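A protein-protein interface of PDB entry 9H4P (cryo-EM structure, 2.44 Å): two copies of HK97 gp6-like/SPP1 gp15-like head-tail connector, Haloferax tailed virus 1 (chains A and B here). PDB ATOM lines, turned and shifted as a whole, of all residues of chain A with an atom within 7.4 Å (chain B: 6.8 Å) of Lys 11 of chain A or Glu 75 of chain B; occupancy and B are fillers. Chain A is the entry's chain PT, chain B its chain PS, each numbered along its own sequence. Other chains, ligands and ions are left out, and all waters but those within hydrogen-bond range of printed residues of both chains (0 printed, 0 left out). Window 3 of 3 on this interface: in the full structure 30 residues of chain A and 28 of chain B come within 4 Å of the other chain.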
ATOM      1  N   VAL A   9     -13.873 -13.037  41.052  1.00  0.00           N
ATOM      2  CA  VAL A   9     -13.146 -14.155  40.451  1.00  0.00           C
ATOM      3  C   VAL A   9     -12.723 -13.836  39.012  1.00  0.00           C
ATOM      4  O   VAL A   9     -13.496 -13.266  38.245  1.00  0.00           O
ATOM      5  CB  VAL A   9     -13.944 -15.477  40.515  1.00  0.00           C
ATOM      6  CG1 VAL A   9     -13.999 -16.059  41.917  1.00  0.00           C
ATOM      7  CG2 VAL A   9     -15.342 -15.373  39.922  1.00  0.00           C
ATOM      8  N   SER A  10     -11.486 -14.229  38.659  1.00  0.00           N
ATOM      9  CA  SER A  10     -10.970 -14.259  37.293  1.00  0.00           C
ATOM     10  C   SER A  10     -11.100 -15.678  36.728  1.00  0.00           C
ATOM     11  O   SER A  10     -11.559 -16.567  37.441  1.00  0.00           O
ATOM     12  CB  SER A  10      -9.547 -13.759  37.257  1.00  0.00           C
ATOM     13  OG  SER A  10      -9.123 -13.523  35.925  1.00  0.00           O
ATOM     14  N   LYS A  11     -10.710 -15.891  35.458  1.00  0.00           N
ATOM     15  CA  LYS A  11     -10.897 -17.151  34.738  1.00  0.00           C
ATOM     16  C   LYS A  11     -10.255 -18.333  35.471  1.00  0.00           C
ATOM     17  O   LYS A  11     -10.881 -19.383  35.594  1.00  0.00           O
ATOM     18  CB  LYS A  11     -10.401 -17.041  33.293  1.00  0.00           C
ATOM     19  CG  LYS A  11     -10.734 -18.230  32.399  1.00  0.00           C
ATOM     20  CD  LYS A  11     -10.183 -18.128  30.994  1.00  0.00           C
ATOM     21  CE  LYS A  11      -8.674 -18.219  30.923  1.00  0.00           C
ATOM     22  NZ  LYS A  11      -8.188 -18.273  29.525  1.00  0.00           N
ATOM     23  N   SER A  12      -9.009 -18.155  35.939  1.00  0.00           N
ATOM     24  CA  SER A  12      -8.265 -19.161  36.688  1.00  0.00           C
ATOM     25  C   SER A  12      -8.888 -19.441  38.058  1.00  0.00           C
ATOM     26  O   SER A  12      -8.776 -20.558  38.560  1.00  0.00           O
ATOM     27  CB  SER A  12      -6.805 -18.792  36.807  1.00  0.00           C
ATOM     28  OG  SER A  12      -6.641 -17.522  37.422  1.00  0.00           O
ATOM     29  N   ASP A  13      -9.536 -18.428  38.657  1.00  0.00           N
ATOM     30  CA  ASP A  13     -10.228 -18.551  39.935  1.00  0.00           C
ATOM     31  C   ASP A  13     -11.540 -19.323  39.772  1.00  0.00           C
ATOM     32  O   ASP A  13     -11.902 -20.104  40.649  1.00  0.00           O
ATOM     33  CB  ASP A  13     -10.477 -17.189  40.594  1.00  0.00           C
ATOM     34  CG  ASP A  13      -9.263 -16.279  40.686  1.00  0.00           C
ATOM     35  OD1 ASP A  13      -8.180 -16.773  41.033  1.00  0.00           O
ATOM     36  OD2 ASP A  13      -9.419 -15.075  40.423  1.00  0.00           O
ATOM     37  N   TRP A  14     -12.251 -19.075  38.662  1.00  0.00           N
ATOM     38  CA  TRP A  14     -13.496 -19.753  38.325  1.00  0.00           C
ATOM     39  C   TRP A  14     -13.269 -21.261  38.207  1.00  0.00           C
ATOM     40  O   TRP A  14     -14.106 -22.041  38.653  1.00  0.00           O
ATOM     41  CB  TRP A  14     -14.107 -19.153  37.049  1.00  0.00           C
ATOM     42  CG  TRP A  14     -15.245 -19.932  36.457  1.00  0.00           C
ATOM     43  CD1 TRP A  14     -15.165 -20.895  35.493  1.00  0.00           C
ATOM     44  CD2 TRP A  14     -16.645 -19.825  36.790  1.00  0.00           C
ATOM     45  NE1 TRP A  14     -16.409 -21.390  35.205  1.00  0.00           N
ATOM     46  CE2 TRP A  14     -17.341 -20.755  35.985  1.00  0.00           C
ATOM     47  CE3 TRP A  14     -17.384 -19.041  37.687  1.00  0.00           C
ATOM     48  CZ2 TRP A  14     -18.730 -20.906  36.046  1.00  0.00           C
ATOM     49  CZ3 TRP A  14     -18.754 -19.200  37.757  1.00  0.00           C
ATOM     50  CH2 TRP A  14     -19.420 -20.122  36.946  1.00  0.00           C
ATOM     51  N   ASP A  15     -12.133 -21.652  37.610  1.00  0.00           N
ATOM     52  CA  ASP A  15     -11.721 -23.039  37.463  1.00  0.00           C
ATOM     53  C   ASP A  15     -11.371 -23.661  38.821  1.00  0.00           C
ATOM     54  O   ASP A  15     -11.387 -24.884  38.944  1.00  0.00           O
ATOM     55  CB  ASP A  15     -10.560 -23.175  36.469  1.00  0.00           C
ATOM     56  CG  ASP A  15     -10.900 -22.904  35.011  1.00  0.00           C
ATOM     57  OD1 ASP A  15     -12.096 -22.880  34.669  1.00  0.00           O
ATOM     58  OD2 ASP A  15      -9.954 -22.732  34.222  1.00  0.00           O
ATOM     59  N   ALA A  16     -11.069 -22.825  39.830  1.00  0.00           N
ATOM     60  CA  ALA A  16     -10.688 -23.266  41.168  1.00  0.00           C
ATOM     61  C   ALA A  16     -11.878 -23.351  42.131  1.00  0.00           C
ATOM     62  O   ALA A  16     -11.726 -23.925  43.208  1.00  0.00           O
ATOM     63  CB  ALA A  16      -9.587 -22.388  41.715  1.00  0.00           C
ATOM     64  N   LEU A  17     -13.050 -22.797  41.767  1.00  0.00           N
ATOM     65  CA  LEU A  17     -14.249 -22.833  42.602  1.00  0.00           C
ATOM     66  C   LEU A  17     -14.728 -24.272  42.799  1.00  0.00           C
ATOM     67  O   LEU A  17     -14.552 -25.103  41.913  1.00  0.00           O
ATOM     68  CB  LEU A  17     -15.368 -22.008  41.949  1.00  0.00           C
ATOM     69  CG  LEU A  17     -15.199 -20.488  41.909  1.00  0.00           C
ATOM     70  CD1 LEU A  17     -16.389 -19.840  41.223  1.00  0.00           C
ATOM     71  CD2 LEU A  17     -15.016 -19.900  43.298  1.00  0.00           C
ATOM     72  N   GLU A  47     -19.599 -22.386  30.451  1.00  0.00           N
ATOM     73  CA  GLU A  47     -18.731 -21.892  29.386  1.00  0.00           C
ATOM     74  C   GLU A  47     -19.001 -20.414  29.094  1.00  0.00           C
ATOM     75  O   GLU A  47     -18.054 -19.648  28.927  1.00  0.00           O
ATOM     76  CB  GLU A  47     -18.902 -22.729  28.114  1.00  0.00           C
ATOM     77  CG  GLU A  47     -17.751 -22.588  27.135  1.00  0.00           C
ATOM     78  CD  GLU A  47     -16.504 -23.358  27.526  1.00  0.00           C
ATOM     79  OE1 GLU A  47     -16.608 -24.581  27.732  1.00  0.00           O
ATOM     80  OE2 GLU A  47     -15.437 -22.733  27.628  1.00  0.00           O
ATOM     81  N   ARG A  50     -17.675 -18.327  32.113  1.00  0.00           N
ATOM     82  CA  ARG A  50     -16.219 -18.346  32.060  1.00  0.00           C
ATOM     83  C   ARG A  50     -15.701 -17.415  30.959  1.00  0.00           C
ATOM     84  O   ARG A  50     -14.681 -16.748  31.143  1.00  0.00           O
ATOM     85  CB  ARG A  50     -15.740 -19.791  31.880  1.00  0.00           C
ATOM     86  CG  ARG A  50     -14.241 -19.993  32.041  1.00  0.00           C
ATOM     87  CD  ARG A  50     -13.917 -21.468  31.935  1.00  0.00           C
ATOM     88  NE  ARG A  50     -12.508 -21.777  32.140  1.00  0.00           N
ATOM     89  CZ  ARG A  50     -11.574 -21.819  31.193  1.00  0.00           C
ATOM     90  NH1 ARG A  50     -10.330 -22.125  31.517  1.00  0.00           N
ATOM     91  NH2 ARG A  50     -11.875 -21.557  29.933  1.00  0.00           N
ATOM     92  N   SER A  51     -16.418 -17.379  29.824  1.00  0.00           N
ATOM     93  CA  SER A  51     -16.088 -16.530  28.688  1.00  0.00           C
ATOM     94  C   SER A  51     -16.388 -15.062  28.989  1.00  0.00           C
ATOM     95  O   SER A  51     -15.652 -14.186  28.533  1.00  0.00           O
ATOM     96  CB  SER A  51     -16.812 -16.989  27.450  1.00  0.00           C
ATOM     97  OG  SER A  51     -16.316 -16.325  26.297  1.00  0.00           O
ATOM     98  N   ILE A  53     -16.308 -13.747  32.039  1.00  0.00           N
ATOM     99  CA  ILE A  53     -15.256 -13.409  32.988  1.00  0.00           C
ATOM    100  C   ILE A  53     -13.969 -13.057  32.232  1.00  0.00           C
ATOM    101  O   ILE A  53     -13.321 -12.063  32.562  1.00  0.00           O
ATOM    102  CB  ILE A  53     -15.077 -14.539  34.028  1.00  0.00           C
ATOM    103  CG1 ILE A  53     -16.259 -14.598  35.002  1.00  0.00           C
ATOM    104  CG2 ILE A  53     -13.761 -14.405  34.776  1.00  0.00           C
ATOM    105  CD1 ILE A  53     -16.381 -15.892  35.775  1.00  0.00           C
ATOM    106  N   ALA A  54     -13.622 -13.868  31.217  1.00  0.00           N
ATOM    107  CA  ALA A  54     -12.448 -13.658  30.380  1.00  0.00           C
ATOM    108  C   ALA A  54     -12.518 -12.322  29.638  1.00  0.00           C
ATOM    109  O   ALA A  54     -11.519 -11.608  29.590  1.00  0.00           O
ATOM    110  CB  ALA A  54     -12.278 -14.816  29.427  1.00  0.00           C
ATOM    111  N   GLU A  55     -13.689 -11.989  29.069  1.00  0.00           N
ATOM    112  CA  GLU A  55     -13.872 -10.752  28.322  1.00  0.00           C
ATOM    113  C   GLU A  55     -13.885  -9.526  29.233  1.00  0.00           C
ATOM    114  O   GLU A  55     -13.362  -8.488  28.839  1.00  0.00           O
ATOM    115  CB  GLU A  55     -15.132 -10.807  27.466  1.00  0.00           C
ATOM    116  CG  GLU A  55     -14.932 -11.605  26.201  1.00  0.00           C
ATOM    117  CD  GLU A  55     -16.164 -11.711  25.329  1.00  0.00           C
ATOM    118  OE1 GLU A  55     -17.068 -10.871  25.468  1.00  0.00           O
ATOM    119  OE2 GLU A  55     -16.224 -12.642  24.518  1.00  0.00           O
ATOM    120  N   ARG A  56     -14.491  -9.636  30.424  1.00  0.00           N
ATOM    121  CA  ARG A  56     -14.439  -8.563  31.409  1.00  0.00           C
ATOM    122  C   ARG A  56     -12.985  -8.232  31.749  1.00  0.00           C
ATOM    123  O   ARG A  56     -12.608  -7.062  31.756  1.00  0.00           O
ATOM    124  CB  ARG A  56     -15.237  -8.929  32.662  1.00  0.00           C
ATOM    125  CG  ARG A  56     -15.286  -7.827  33.713  1.00  0.00           C
ATOM    126  CD  ARG A  56     -15.673  -8.368  35.077  1.00  0.00           C
ATOM    127  NE  ARG A  56     -14.623  -9.241  35.589  1.00  0.00           N
ATOM    128  CZ  ARG A  56     -14.799 -10.318  36.348  1.00  0.00           C
ATOM    129  NH1 ARG A  56     -13.747 -11.020  36.728  1.00  0.00           N
ATOM    130  NH2 ARG A  56     -16.008 -10.697  36.719  1.00  0.00           N
ATOM    131  N   ASP A  57     -12.178  -9.269  32.010  1.00  0.00           N
ATOM    132  CA  ASP A  57     -10.798  -9.118  32.449  1.00  0.00           C
ATOM    133  C   ASP A  57      -9.852  -8.720  31.308  1.00  0.00           C
ATOM    134  O   ASP A  57      -8.748  -8.252  31.586  1.00  0.00           O
ATOM    135  CB  ASP A  57     -10.326 -10.363  33.208  1.00  0.00           C
ATOM    136  CG  ASP A  57     -11.018 -10.607  34.539  1.00  0.00           C
ATOM    137  OD1 ASP A  57     -11.851  -9.779  34.947  1.00  0.00           O
ATOM    138  OD2 ASP A  57     -10.707 -11.627  35.162  1.00  0.00           O
ATOM    139  N   PRO B   2      -9.471 -28.213  28.578  1.00  0.00           N
ATOM    140  CA  PRO B   2      -8.541 -29.167  27.961  1.00  0.00           C
ATOM    141  C   PRO B   2      -7.129 -29.043  28.535  1.00  0.00           C
ATOM    142  O   PRO B   2      -6.772 -27.992  29.061  1.00  0.00           O
ATOM    143  CB  PRO B   2      -8.597 -28.798  26.474  1.00  0.00           C
ATOM    144  CG  PRO B   2     -10.025 -28.381  26.284  1.00  0.00           C
ATOM    145  CD  PRO B   2     -10.352 -27.638  27.558  1.00  0.00           C
ATOM    146  N   SER B   5      -4.451 -26.261  25.932  1.00  0.00           N
ATOM    147  CA  SER B   5      -5.520 -25.328  25.604  1.00  0.00           C
ATOM    148  C   SER B   5      -5.397 -24.871  24.149  1.00  0.00           C
ATOM    149  O   SER B   5      -4.297 -24.859  23.605  1.00  0.00           O
ATOM    150  CB  SER B   5      -5.511 -24.170  26.566  1.00  0.00           C
ATOM    151  OG  SER B   5      -6.595 -23.294  26.309  1.00  0.00           O
ATOM    152  N   ILE B   6      -6.523 -24.465  23.540  1.00  0.00           N
ATOM    153  CA  ILE B   6      -6.633 -24.138  22.120  1.00  0.00           C
ATOM    154  C   ILE B   6      -5.740 -22.948  21.729  1.00  0.00           C
ATOM    155  O   ILE B   6      -5.370 -22.822  20.563  1.00  0.00           O
ATOM    156  CB  ILE B   6      -8.115 -23.966  21.707  1.00  0.00           C
ATOM    157  CG1 ILE B   6      -8.307 -23.971  20.186  1.00  0.00           C
ATOM    158  CG2 ILE B   6      -8.746 -22.749  22.371  1.00  0.00           C
ATOM    159  CD1 ILE B   6      -9.747 -23.985  19.719  1.00  0.00           C
ATOM    160  N   ASP B   7      -5.375 -22.099  22.705  1.00  0.00           N
ATOM    161  CA  ASP B   7      -4.502 -20.949  22.496  1.00  0.00           C
ATOM    162  C   ASP B   7      -3.019 -21.332  22.535  1.00  0.00           C
ATOM    163  O   ASP B   7      -2.179 -20.540  22.111  1.00  0.00           O
ATOM    164  CB  ASP B   7      -4.800 -19.815  23.482  1.00  0.00           C
ATOM    165  CG  ASP B   7      -4.747 -20.203  24.949  1.00  0.00           C
ATOM    166  OD1 ASP B   7      -5.321 -21.241  25.306  1.00  0.00           O
ATOM    167  OD2 ASP B   7      -4.144 -19.448  25.727  1.00  0.00           O
ATOM    168  N   GLN B  28     -15.111 -28.610  23.976  1.00  0.00           N
ATOM    169  CA  GLN B  28     -15.190 -27.231  24.439  1.00  0.00           C
ATOM    170  C   GLN B  28     -15.896 -26.350  23.407  1.00  0.00           C
ATOM    171  O   GLN B  28     -16.689 -25.491  23.791  1.00  0.00           O
ATOM    172  CB  GLN B  28     -13.830 -26.657  24.844  1.00  0.00           C
ATOM    173  CG  GLN B  28     -13.955 -25.328  25.580  1.00  0.00           C
ATOM    174  CD  GLN B  28     -12.670 -24.747  26.111  1.00  0.00           C
ATOM    175  OE1 GLN B  28     -11.573 -25.191  25.787  1.00  0.00           O
ATOM    176  NE2 GLN B  28     -12.798 -23.720  26.933  1.00  0.00           N
ATOM    177  N   ARG B  56      -5.944 -17.670  12.882  1.00  0.00           N
ATOM    178  CA  ARG B  56      -5.481 -16.878  14.016  1.00  0.00           C
ATOM    179  C   ARG B  56      -3.989 -16.576  13.866  1.00  0.00           C
ATOM    180  O   ARG B  56      -3.583 -15.421  13.957  1.00  0.00           O
ATOM    181  CB  ARG B  56      -5.781 -17.591  15.342  1.00  0.00           C
ATOM    182  CG  ARG B  56      -5.277 -16.884  16.595  1.00  0.00           C
ATOM    183  CD  ARG B  56      -5.210 -17.847  17.768  1.00  0.00           C
ATOM    184  NE  ARG B  56      -4.115 -18.797  17.607  1.00  0.00           N
ATOM    185  CZ  ARG B  56      -4.043 -20.018  18.133  1.00  0.00           C
ATOM    186  NH1 ARG B  56      -2.980 -20.765  17.891  1.00  0.00           N
ATOM    187  NH2 ARG B  56      -5.016 -20.495  18.888  1.00  0.00           N
ATOM    188  N   LEU B  70      -4.454  -9.291  18.580  1.00  0.00           N
ATOM    189  CA  LEU B  70      -5.400 -10.057  19.375  1.00  0.00           C
ATOM    190  C   LEU B  70      -5.326  -9.575  20.829  1.00  0.00           C
ATOM    191  O   LEU B  70      -4.462 -10.005  21.595  1.00  0.00           O
ATOM    192  CB  LEU B  70      -5.076 -11.548  19.206  1.00  0.00           C
ATOM    193  CG  LEU B  70      -5.915 -12.546  20.004  1.00  0.00           C
ATOM    194  CD1 LEU B  70      -7.404 -12.311  19.811  1.00  0.00           C
ATOM    195  CD2 LEU B  70      -5.555 -13.968  19.618  1.00  0.00           C
ATOM    196  N   GLY B  72      -8.038  -9.511  23.114  1.00  0.00           N
ATOM    197  CA  GLY B  72      -8.840 -10.343  24.001  1.00  0.00           C
ATOM    198  C   GLY B  72      -8.195 -11.698  24.287  1.00  0.00           C
ATOM    199  O   GLY B  72      -7.097 -11.972  23.808  1.00  0.00           O
ATOM    200  N   ASP B  73      -8.892 -12.540  25.064  1.00  0.00           N
ATOM    201  CA  ASP B  73      -8.408 -13.860  25.450  1.00  0.00           C
ATOM    202  C   ASP B  73      -8.335 -14.779  24.229  1.00  0.00           C
ATOM    203  O   ASP B  73      -9.364 -15.104  23.641  1.00  0.00           O
ATOM    204  CB  ASP B  73      -9.277 -14.466  26.557  1.00  0.00           C
ATOM    205  CG  ASP B  73      -8.774 -15.784  27.127  1.00  0.00           C
ATOM    206  OD1 ASP B  73      -7.765 -16.312  26.626  1.00  0.00           O
ATOM    207  OD2 ASP B  73      -9.395 -16.265  28.087  1.00  0.00           O
ATOM    208  N   ALA B  74      -7.115 -15.234  23.902  1.00  0.00           N
ATOM    209  CA  ALA B  74      -6.833 -16.062  22.736  1.00  0.00           C
ATOM    210  C   ALA B  74      -7.567 -17.407  22.769  1.00  0.00           C
ATOM    211  O   ALA B  74      -7.822 -17.975  21.708  1.00  0.00           O
ATOM    212  CB  ALA B  74      -5.342 -16.241  22.582  1.00  0.00           C
ATOM    213  N   GLU B  75      -7.892 -17.918  23.969  1.00  0.00           N
ATOM    214  CA  GLU B  75      -8.680 -19.135  24.123  1.00  0.00           C
ATOM    215  C   GLU B  75     -10.048 -18.930  23.474  1.00  0.00           C
ATOM    216  O   GLU B  75     -10.363 -19.592  22.487  1.00  0.00           O
ATOM    217  CB  GLU B  75      -8.764 -19.551  25.596  1.00  0.00           C
ATOM    218  CG  GLU B  75      -9.567 -20.817  25.856  1.00  0.00           C
ATOM    219  CD  GLU B  75      -9.708 -21.208  27.317  1.00  0.00           C
ATOM    220  OE1 GLU B  75      -9.101 -20.543  28.173  1.00  0.00           O
ATOM    221  OE2 GLU B  75     -10.427 -22.184  27.589  1.00  0.00           O
ATOM    222  N   TYR B  76     -10.820 -17.973  24.008  1.00  0.00           N
ATOM    223  CA  TYR B  76     -12.174 -17.707  23.544  1.00  0.00           C
ATOM    224  C   TYR B  76     -12.214 -17.131  22.133  1.00  0.00           C
ATOM    225  O   TYR B  76     -13.194 -17.362  21.431  1.00  0.00           O
ATOM    226  CB  TYR B  76     -12.981 -16.928  24.583  1.00  0.00           C
ATOM    227  CG  TYR B  76     -13.390 -17.835  25.707  1.00  0.00           C
ATOM    228  CD1 TYR B  76     -14.349 -18.813  25.500  1.00  0.00           C
ATOM    229  CD2 TYR B  76     -12.757 -17.790  26.939  1.00  0.00           C
ATOM    230  CE1 TYR B  76     -14.706 -19.700  26.501  1.00  0.00           C
ATOM    231  CE2 TYR B  76     -13.104 -18.667  27.954  1.00  0.00           C
ATOM    232  CZ  TYR B  76     -14.082 -19.624  27.733  1.00  0.00           C
ATOM    233  OH  TYR B  76     -14.441 -20.494  28.720  1.00  0.00           O
ATOM    234  N   PHE B  77     -11.167 -16.403  21.719  1.00  0.00           N
ATOM    235  CA  PHE B  77     -11.077 -15.973  20.332  1.00  0.00           C
ATOM    236  C   PHE B  77     -11.030 -17.180  19.399  1.00  0.00           C
ATOM    237  O   PHE B  77     -11.789 -17.217  18.434  1.00  0.00           O
ATOM    238  CB  PHE B  77      -9.879 -15.057  20.070  1.00  0.00           C
ATOM    239  CG  PHE B  77      -9.765 -14.663  18.619  1.00  0.00           C
ATOM    240  CD1 PHE B  77     -10.692 -13.797  18.053  1.00  0.00           C
ATOM    241  CD2 PHE B  77      -8.770 -15.190  17.806  1.00  0.00           C
ATOM    242  CE1 PHE B  77     -10.619 -13.453  16.712  1.00  0.00           C
ATOM    243  CE2 PHE B  77      -8.693 -14.842  16.464  1.00  0.00           C
ATOM    244  CZ  PHE B  77      -9.615 -13.971  15.923  1.00  0.00           C
ATOM    245  N   THR B  78     -10.147 -18.150  19.688  1.00  0.00           N
ATOM    246  CA  THR B  78      -9.995 -19.317  18.830  1.00  0.00           C
ATOM    247  C   THR B  78     -11.263 -20.171  18.841  1.00  0.00           C
ATOM    248  O   THR B  78     -11.624 -20.722  17.803  1.00  0.00           O
ATOM    249  CB  THR B  78      -8.759 -20.166  19.153  1.00  0.00           C
ATOM    250  OG1 THR B  78      -7.670 -19.332  19.541  1.00  0.00           O
ATOM    251  CG2 THR B  78      -8.320 -20.994  17.967  1.00  0.00           C
ATOM    252  N   LEU B  79     -11.926 -20.273  20.003  1.00  0.00           N
ATOM    253  CA  LEU B  79     -13.192 -20.987  20.125  1.00  0.00           C
ATOM    254  C   LEU B  79     -14.279 -20.327  19.273  1.00  0.00           C
ATOM    255  O   LEU B  79     -14.948 -21.019  18.509  1.00  0.00           O
ATOM    256  CB  LEU B  79     -13.613 -21.113  21.594  1.00  0.00           C
ATOM    257  CG  LEU B  79     -12.703 -21.952  22.496  1.00  0.00           C
ATOM    258  CD1 LEU B  79     -13.064 -21.762  23.957  1.00  0.00           C
ATOM    259  CD2 LEU B  79     -12.752 -23.428  22.140  1.00  0.00           C
ATOM    260  N   TYR B  80     -14.448 -18.999  19.394  1.00  0.00           N
ATOM    261  CA  TYR B  80     -15.460 -18.273  18.631  1.00  0.00           C
ATOM    262  C   TYR B  80     -15.186 -18.315  17.128  1.00  0.00           C
ATOM    263  O   TYR B  80     -16.132 -18.431  16.351  1.00  0.00           O
ATOM    264  CB  TYR B  80     -15.669 -16.845  19.150  1.00  0.00           C
ATOM    265  CG  TYR B  80     -16.330 -16.776  20.504  1.00  0.00           C
ATOM    266  CD1 TYR B  80     -17.490 -17.493  20.770  1.00  0.00           C
ATOM    267  CD2 TYR B  80     -15.803 -15.994  21.520  1.00  0.00           C
ATOM    268  CE1 TYR B  80     -18.094 -17.458  22.016  1.00  0.00           C
ATOM    269  CE2 TYR B  80     -16.397 -15.943  22.772  1.00  0.00           C
ATOM    270  CZ  TYR B  80     -17.546 -16.678  23.018  1.00  0.00           C
ATOM    271  OH  TYR B  80     -18.149 -16.642  24.241  1.00  0.00           O
ATOM    272  N   TYR B 128     -12.550  -8.987  19.812  1.00  0.00           N
ATOM    273  CA  TYR B 128     -11.238  -9.360  20.342  1.00  0.00           C
ATOM    274  C   TYR B 128     -10.092  -8.741  19.534  1.00  0.00           C
ATOM    275  O   TYR B 128      -8.963  -8.694  20.021  1.00  0.00           O
ATOM    276  CB  TYR B 128     -11.047 -10.882  20.353  1.00  0.00           C
ATOM    277  CG  TYR B 128     -11.833 -11.666  21.378  1.00  0.00           C
ATOM    278  CD1 TYR B 128     -13.220 -11.683  21.361  1.00  0.00           C
ATOM    279  CD2 TYR B 128     -11.191 -12.431  22.340  1.00  0.00           C
ATOM    280  CE1 TYR B 128     -13.948 -12.410  22.289  1.00  0.00           C
ATOM    281  CE2 TYR B 128     -11.903 -13.165  23.277  1.00  0.00           C
ATOM    282  CZ  TYR B 128     -13.285 -13.151  23.251  1.00  0.00           C
ATOM    283  OH  TYR B 128     -13.990 -13.874  24.165  1.00  0.00           O
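The side-chain carboxylate (OD2) of Asp 73 of chain B lies within salt-bridge range of the side-chain amino group (NZ) of Lys 11 of chain A (2.7 Å). The side-chain amino group (NZ) of Lys 11 of chain A lies within salt-bridge range of the side-chain carboxylate (OE1) of Glu 75 of chain B. The side-chain amide nitrogen (NE2) of Gln 28 of chain B is in hydrogen-bond range of the side-chain carboxylate (OE2) of Glu 47 of chain A (2.9 Å). The side-chain carboxylate (OE2) of Glu 47 of chain A sits at hydrogen-bond distance from the side-chain hydroxyl (OH) of Tyr 76 of chain B, at 2.7 Å. NH2 of Arg 50 of chain A is in salt-bridge range of OE2 of Glu 75 of chain B (2.8 Å). The side-chain hydroxyl (OH) of Tyr 76 of chain B lies within hydrogen-bond range of the guanidinium group (NH2) of Arg 50 of chain A. OG of Ser 51 of chain A sits at hydrogen-bond distance from OH of Tyr 80 of chain B (2.8 Å). The side-chain carboxylate of Glu 55 of chain A lies within hydrogen-bond range of the side-chain hydroxyl of Tyr 128 of chain B (2.6 Å).
The side-chain carboxylate of Asp 15 of chain A lies within salt-bridge range of the guanidinium group of Arg 50 of chain A, at 2.8 Å. OE2 of Glu 75 of chain B lies within hydrogen-bond range of NE2 of Gln 28 of chain B. O of Tyr 128 of chain B lies within hydrogen-bond range of N of Gly 72 of chain B (3.3 Å). The side-chain carboxylate (OD1) of Asp 73 of chain B sits at hydrogen-bond distance from the backbone NH (N) of Glu 75 of chain B, at 3.1 Å.
Among the printed residues, pairs that only touch across the chains: Ser 51 of chain A with Tyr 76 of chain B, Ala 54 of chain A with Asp 73 of chain B, Glu 55 of chain A with Tyr 80 of chain B, Arg 50 of chain A with Gln 28 of chain B, Ala 54 of chain A with Tyr 76 of chain B and Ser 51 of chain A with Tyr 128 of chain B.
Of the printed residues of chain B, Lys 11 of chain A touches Asp 73 (2.7 Å) and Glu 75 (2.8 Å). Of chain A, only Lys 11 (2.8 Å) and Arg 50 (2.8 Å) come within 4 Å of Glu 75 of chain B. Of the printed residues of chain A, Asp 73 of chain B touches Lys 11 and Ala 54. Printed residues of chain B within 4 Å of Ser 51 of chain A: Tyr 76 (3.3 Å), Tyr 80 (2.8 Å) and Tyr 128 (3.995 Å). Printed residues of chain B within 4 Å of Glu 55 of chain A: Tyr 80 (3.7 Å) and Tyr 128 (2.6 Å). The nearest residue of chain B that does not touch Lys 11 of chain A is Tyr 76 of chain B (4.3 Å). The nearest printed residue of chain B that does not touch Glu 47 of chain A is Leu 79 of chain B (4.5 Å).
Of the 17 printed residues of chain B, 6 touch a printed residue of chain A. Among the printed residues, 14 pairs touch across the chains.
1 position is printed for both chains. Of the 14 pairs that touch across the chains among the printed residues, none has its exchanged pair printed and touching as well.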
